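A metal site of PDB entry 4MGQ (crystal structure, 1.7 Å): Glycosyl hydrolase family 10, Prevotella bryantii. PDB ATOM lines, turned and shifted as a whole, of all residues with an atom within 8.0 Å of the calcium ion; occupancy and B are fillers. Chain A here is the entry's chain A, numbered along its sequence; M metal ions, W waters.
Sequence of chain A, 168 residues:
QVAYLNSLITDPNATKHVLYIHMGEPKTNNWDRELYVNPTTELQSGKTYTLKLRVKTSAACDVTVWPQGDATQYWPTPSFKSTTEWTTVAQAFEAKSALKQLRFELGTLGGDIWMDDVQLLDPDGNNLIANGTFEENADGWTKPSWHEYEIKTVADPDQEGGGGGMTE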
ATOM      1  N   THR A  15       6.969  20.343  -0.924  1.00  0.00           N
ATOM      2  CA  THR A  15       6.964  20.601  -2.365  1.00  0.00           C
ATOM      3  C   THR A  15       5.919  19.745  -3.054  1.00  0.00           C
ATOM      4  O   THR A  15       5.888  18.513  -2.877  1.00  0.00           O
ATOM      5  CB  THR A  15       8.332  20.336  -2.984  1.00  0.00           C
ATOM      6  OG1 THR A  15       9.321  21.074  -2.261  1.00  0.00           O
ATOM      7  CG2 THR A  15       8.343  20.767  -4.456  1.00  0.00           C
ATOM      8  N   LYS A  16       5.049  20.398  -3.820  1.00  0.00           N
ATOM      9  CA  LYS A  16       4.055  19.732  -4.647  1.00  0.00           C
ATOM     10  C   LYS A  16       4.613  19.655  -6.058  1.00  0.00           C
ATOM     11  O   LYS A  16       5.380  20.528  -6.465  1.00  0.00           O
ATOM     12  CB  LYS A  16       2.733  20.493  -4.659  1.00  0.00           C
ATOM     13  CG  LYS A  16       2.057  20.673  -3.312  1.00  0.00           C
ATOM     14  CD  LYS A  16       0.854  21.602  -3.464  1.00  0.00           C
ATOM     15  CE  LYS A  16      -0.117  21.463  -2.300  1.00  0.00           C
ATOM     16  NZ  LYS A  16       0.275  22.262  -1.096  1.00  0.00           N
ATOM     17  N   HIS A  17       4.239  18.617  -6.800  1.00  0.00           N
ATOM     18  CA  HIS A  17       4.707  18.501  -8.192  1.00  0.00           C
ATOM     19  C   HIS A  17       3.533  18.481  -9.141  1.00  0.00           C
ATOM     20  O   HIS A  17       2.450  17.994  -8.809  1.00  0.00           O
ATOM     21  CB  HIS A  17       5.586  17.252  -8.356  1.00  0.00           C
ATOM     22  CG  HIS A  17       6.787  17.280  -7.467  1.00  0.00           C
ATOM     23  ND1 HIS A  17       6.769  16.765  -6.183  1.00  0.00           N
ATOM     24  CD2 HIS A  17       8.021  17.813  -7.649  1.00  0.00           C
ATOM     25  CE1 HIS A  17       7.957  16.950  -5.630  1.00  0.00           C
ATOM     26  NE2 HIS A  17       8.724  17.588  -6.487  1.00  0.00           N
ATOM     27  N   VAL A  18       3.742  19.073 -10.318  1.00  0.00           N
ATOM     28  CA  VAL A  18       2.661  19.269 -11.270  1.00  0.00           C
ATOM     29  C   VAL A  18       3.141  18.931 -12.677  1.00  0.00           C
ATOM     30  O   VAL A  18       4.349  18.894 -12.939  1.00  0.00           O
ATOM     31  CB  VAL A  18       2.124  20.718 -11.227  1.00  0.00           C
ATOM     32  CG1 VAL A  18       1.783  21.139  -9.788  1.00  0.00           C
ATOM     33  CG2 VAL A  18       3.157  21.682 -11.812  1.00  0.00           C
ATOM     34  N   LEU A  19       2.199  18.667 -13.575  1.00  0.00           N
ATOM     35  CA  LEU A  19       2.504  18.538 -14.990  1.00  0.00           C
ATOM     36  C   LEU A  19       2.794  19.935 -15.542  1.00  0.00           C
ATOM     37  O   LEU A  19       2.067  20.882 -15.249  1.00  0.00           O
ATOM     38  CB  LEU A  19       1.335  17.874 -15.738  1.00  0.00           C
ATOM     39  CG  LEU A  19       1.472  17.697 -17.266  1.00  0.00           C
ATOM     40  CD1 LEU A  19       0.581  16.561 -17.723  1.00  0.00           C
ATOM     41  CD2 LEU A  19       1.112  18.955 -18.041  1.00  0.00           C
ATOM     42  N   ARG A  54      -6.716  20.971 -11.214  1.00  0.00           N
ATOM     43  CA  ARG A  54      -6.388  22.379 -11.060  1.00  0.00           C
ATOM     44  C   ARG A  54      -5.451  22.763 -12.192  1.00  0.00           C
ATOM     45  O   ARG A  54      -4.665  21.937 -12.669  1.00  0.00           O
ATOM     46  CB  ARG A  54      -5.778  22.712  -9.688  1.00  0.00           C
ATOM     47  CG  ARG A  54      -4.506  21.976  -9.325  1.00  0.00           C
ATOM     48  CD  ARG A  54      -3.964  22.456  -7.950  1.00  0.00           C
ATOM     49  NE  ARG A  54      -2.702  21.801  -7.670  1.00  0.00           N
ATOM     50  CZ  ARG A  54      -1.597  22.438  -7.285  1.00  0.00           C
ATOM     51  NH1 ARG A  54      -1.620  23.747  -7.068  1.00  0.00           N
ATOM     52  NH2 ARG A  54      -0.479  21.751  -7.074  1.00  0.00           N
ATOM     53  N   TRP A  86      -3.655  29.479  -9.895  1.00  0.00           N
ATOM     54  CA  TRP A  86      -4.274  28.156  -9.805  1.00  0.00           C
ATOM     55  C   TRP A  86      -5.776  28.286  -9.569  1.00  0.00           C
ATOM     56  O   TRP A  86      -6.205  29.015  -8.679  1.00  0.00           O
ATOM     57  CB  TRP A  86      -3.672  27.320  -8.672  1.00  0.00           C
ATOM     58  CG  TRP A  86      -2.315  26.750  -8.912  1.00  0.00           C
ATOM     59  CD1 TRP A  86      -1.157  27.129  -8.305  1.00  0.00           C
ATOM     60  CD2 TRP A  86      -1.981  25.667  -9.787  1.00  0.00           C
ATOM     61  NE1 TRP A  86      -0.110  26.364  -8.748  1.00  0.00           N
ATOM     62  CE2 TRP A  86      -0.596  25.450  -9.651  1.00  0.00           C
ATOM     63  CE3 TRP A  86      -2.713  24.858 -10.655  1.00  0.00           C
ATOM     64  CZ2 TRP A  86       0.075  24.461 -10.366  1.00  0.00           C
ATOM     65  CZ3 TRP A  86      -2.047  23.879 -11.361  1.00  0.00           C
ATOM     66  CH2 TRP A  86      -0.671  23.688 -11.214  1.00  0.00           C
ATOM     67  N   MET A 115      -0.695  21.733 -14.786  1.00  0.00           N
ATOM     68  CA  MET A 115      -1.901  21.037 -14.375  1.00  0.00           C
ATOM     69  C   MET A 115      -1.575  20.067 -13.241  1.00  0.00           C
ATOM     70  O   MET A 115      -0.467  19.559 -13.172  1.00  0.00           O
ATOM     71  CB  MET A 115      -2.554  20.280 -15.545  1.00  0.00           C
ATOM     72  CG  MET A 115      -3.273  21.201 -16.514  1.00  0.00           C
ATOM     73  SD  MET A 115      -4.167  20.304 -17.800  1.00  0.00           S
ATOM     74  CE  MET A 115      -2.793  19.764 -18.788  1.00  0.00           C
ATOM     75  N   ASP A 116      -2.560  19.819 -12.389  1.00  0.00           N
ATOM     76  CA  ASP A 116      -2.352  18.886 -11.269  1.00  0.00           C
ATOM     77  C   ASP A 116      -3.697  18.333 -10.807  1.00  0.00           C
ATOM     78  O   ASP A 116      -4.763  18.875 -11.147  1.00  0.00           O
ATOM     79  CB  ASP A 116      -1.633  19.591 -10.104  1.00  0.00           C
ATOM     80  CG  ASP A 116      -0.982  18.614  -9.129  1.00  0.00           C
ATOM     81  OD1 ASP A 116      -0.806  17.417  -9.459  1.00  0.00           O
ATOM     82  OD2 ASP A 116      -0.608  19.073  -8.020  1.00  0.00           O
ATOM     83  N   ASP A 117      -3.636  17.252 -10.041  1.00  0.00           N
ATOM     84  CA  ASP A 117      -4.815  16.674  -9.412  1.00  0.00           C
ATOM     85  C   ASP A 117      -5.901  16.344 -10.434  1.00  0.00           C
ATOM     86  O   ASP A 117      -7.084  16.616 -10.238  1.00  0.00           O
ATOM     87  CB  ASP A 117      -5.320  17.622  -8.331  1.00  0.00           C
ATOM     88  CG  ASP A 117      -4.246  17.918  -7.290  1.00  0.00           C
ATOM     89  OD1 ASP A 117      -3.659  16.945  -6.780  1.00  0.00           O
ATOM     90  OD2 ASP A 117      -3.974  19.100  -7.008  1.00  0.00           O
ATOM     91  N   VAL A 118      -5.470  15.740 -11.539  1.00  0.00           N
ATOM     92  CA  VAL A 118      -6.371  15.403 -12.628  1.00  0.00           C
ATOM     93  C   VAL A 118      -7.125  14.107 -12.323  1.00  0.00           C
ATOM     94  O   VAL A 118      -6.505  13.062 -12.068  1.00  0.00           O
ATOM     95  CB  VAL A 118      -5.609  15.236 -13.946  1.00  0.00           C
ATOM     96  CG1 VAL A 118      -6.596  15.028 -15.106  1.00  0.00           C
ATOM     97  CG2 VAL A 118      -4.708  16.449 -14.203  1.00  0.00           C
ATOM     98  N   ASN A 131      -2.606   8.439 -13.551  1.00  0.00           N
ATOM     99  CA  ASN A 131      -1.559   9.265 -12.988  1.00  0.00           C
ATOM    100  C   ASN A 131      -1.925  10.742 -13.071  1.00  0.00           C
ATOM    101  O   ASN A 131      -1.574  11.416 -14.029  1.00  0.00           O
ATOM    102  CB  ASN A 131      -0.236   9.005 -13.709  1.00  0.00           C
ATOM    103  CG  ASN A 131       0.873   9.938 -13.267  1.00  0.00           C
ATOM    104  OD1 ASN A 131       0.854  10.477 -12.157  1.00  0.00           O
ATOM    105  ND2 ASN A 131       1.858  10.117 -14.135  1.00  0.00           N
ATOM    106  N   GLY A 132      -2.643  11.216 -12.056  1.00  0.00           N
ATOM    107  CA  GLY A 132      -3.115  12.591 -12.027  1.00  0.00           C
ATOM    108  C   GLY A 132      -2.432  13.462 -10.997  1.00  0.00           C
ATOM    109  O   GLY A 132      -2.744  14.643 -10.885  1.00  0.00           O
ATOM    110  N   THR A 133      -1.504  12.891 -10.226  1.00  0.00           N
ATOM    111  CA  THR A 133      -0.823  13.677  -9.185  1.00  0.00           C
ATOM    112  C   THR A 133       0.601  14.115  -9.517  1.00  0.00           C
ATOM    113  O   THR A 133       1.124  15.029  -8.896  1.00  0.00           O
ATOM    114  CB  THR A 133      -0.751  12.894  -7.848  1.00  0.00           C
ATOM    115  OG1 THR A 133       0.305  11.924  -7.916  1.00  0.00           O
ATOM    116  CG2 THR A 133      -2.065  12.219  -7.576  1.00  0.00           C
ATOM    117  N   PHE A 134       1.251  13.434 -10.465  1.00  0.00           N
ATOM    118  CA  PHE A 134       2.573  13.814 -10.959  1.00  0.00           C
ATOM    119  C   PHE A 134       3.644  13.916  -9.892  1.00  0.00           C
ATOM    120  O   PHE A 134       4.616  14.647 -10.048  1.00  0.00           O
ATOM    121  CB  PHE A 134       2.464  15.139 -11.713  1.00  0.00           C
ATOM    122  CG  PHE A 134       1.372  15.128 -12.732  1.00  0.00           C
ATOM    123  CD1 PHE A 134       1.492  14.379 -13.891  1.00  0.00           C
ATOM    124  CD2 PHE A 134       0.188  15.824 -12.507  1.00  0.00           C
ATOM    125  CE1 PHE A 134       0.478  14.342 -14.820  1.00  0.00           C
ATOM    126  CE2 PHE A 134      -0.832  15.798 -13.441  1.00  0.00           C
ATOM    127  CZ  PHE A 134      -0.691  15.047 -14.595  1.00  0.00           C
ATOM    128  N   GLU A 135       3.495  13.180  -8.794  1.00  0.00           N
ATOM    129  CA  GLU A 135       4.499  13.236  -7.755  1.00  0.00           C
ATOM    130  C   GLU A 135       5.694  12.341  -8.076  1.00  0.00           C
ATOM    131  O   GLU A 135       6.707  12.405  -7.380  1.00  0.00           O
ATOM    132  CB  GLU A 135       3.892  12.858  -6.394  1.00  0.00           C
ATOM    133  CG  GLU A 135       2.828  13.830  -5.925  1.00  0.00           C
ATOM    134  CD  GLU A 135       3.337  15.262  -5.806  1.00  0.00           C
ATOM    135  OE1 GLU A 135       4.453  15.464  -5.274  1.00  0.00           O
ATOM    136  OE2 GLU A 135       2.622  16.192  -6.238  1.00  0.00           O
ATOM    137  N   GLU A 136       5.592  11.526  -9.123  1.00  0.00           N
ATOM    138  CA  GLU A 136       6.720  10.716  -9.557  1.00  0.00           C
ATOM    139  C   GLU A 136       7.156  11.027 -10.989  1.00  0.00           C
ATOM    140  O   GLU A 136       8.335  11.159 -11.271  1.00  0.00           O
ATOM    141  CB  GLU A 136       6.403   9.219  -9.437  1.00  0.00           C
ATOM    142  CG  GLU A 136       6.185   8.750  -8.000  1.00  0.00           C
ATOM    143  CD  GLU A 136       5.769   7.292  -7.917  1.00  0.00           C
ATOM    144  OE1 GLU A 136       4.832   6.879  -8.640  1.00  0.00           O
ATOM    145  OE2 GLU A 136       6.386   6.545  -7.111  1.00  0.00           O
ATOM    146  N   VAL A 154       7.235  19.258 -12.639  1.00  0.00           N
ATOM    147  CA  VAL A 154       8.065  20.256 -11.957  1.00  0.00           C
ATOM    148  C   VAL A 154       7.455  20.595 -10.625  1.00  0.00           C
ATOM    149  O   VAL A 154       6.287  20.321 -10.374  1.00  0.00           O
ATOM    150  CB  VAL A 154       8.212  21.558 -12.772  1.00  0.00           C
ATOM    151  CG1 VAL A 154       8.802  21.286 -14.144  1.00  0.00           C
ATOM    152  CG2 VAL A 154       6.866  22.267 -12.881  1.00  0.00           C
ATOM    153  N   ASP A 156       5.605  22.791  -8.086  1.00  0.00           N
ATOM    154  CA  ASP A 156       4.535  23.790  -8.207  1.00  0.00           C
ATOM    155  C   ASP A 156       5.141  25.203  -8.199  1.00  0.00           C
ATOM    156  O   ASP A 156       5.840  25.579  -7.258  1.00  0.00           O
ATOM    157  CB  ASP A 156       3.531  23.604  -7.060  1.00  0.00           C
ATOM    158  CG  ASP A 156       2.319  24.538  -7.133  1.00  0.00           C
ATOM    159  OD1 ASP A 156       2.410  25.650  -7.686  1.00  0.00           O
ATOM    160  OD2 ASP A 156       1.256  24.156  -6.583  1.00  0.00           O
HETATM  161 CA    CA M   1       0.735  16.968  -7.585  1.00  0.00          CA
HETATM  162  O   HOH W   1       0.644  18.185  -5.472  1.00  0.00           O
HETATM  163  O   HOH W   2      -1.128  15.916  -6.472  1.00  0.00           O
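The backbone carbonyl oxygen of Asp 116 is in hydrogen-bond range of the backbone NH of Arg 54, 2.9 Å away.
The calcium ion is bound by O of His 17 (2.3 Å). The calcium ion is bound by O of Thr 133 (2.4 Å). The calcium ion is bound by water W2 (2.4 Å). Water W1 is bound to the calcium ion. OE2 of Glu 135 is bound to the calcium ion (2.4 Å). The calcium ion is bound by OD1 of Asp 116, 2.5 Å away. OD2 of Asp 116 binds the calcium ion (2.5 Å). The calcium ion has seven donor atoms within binding distance.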
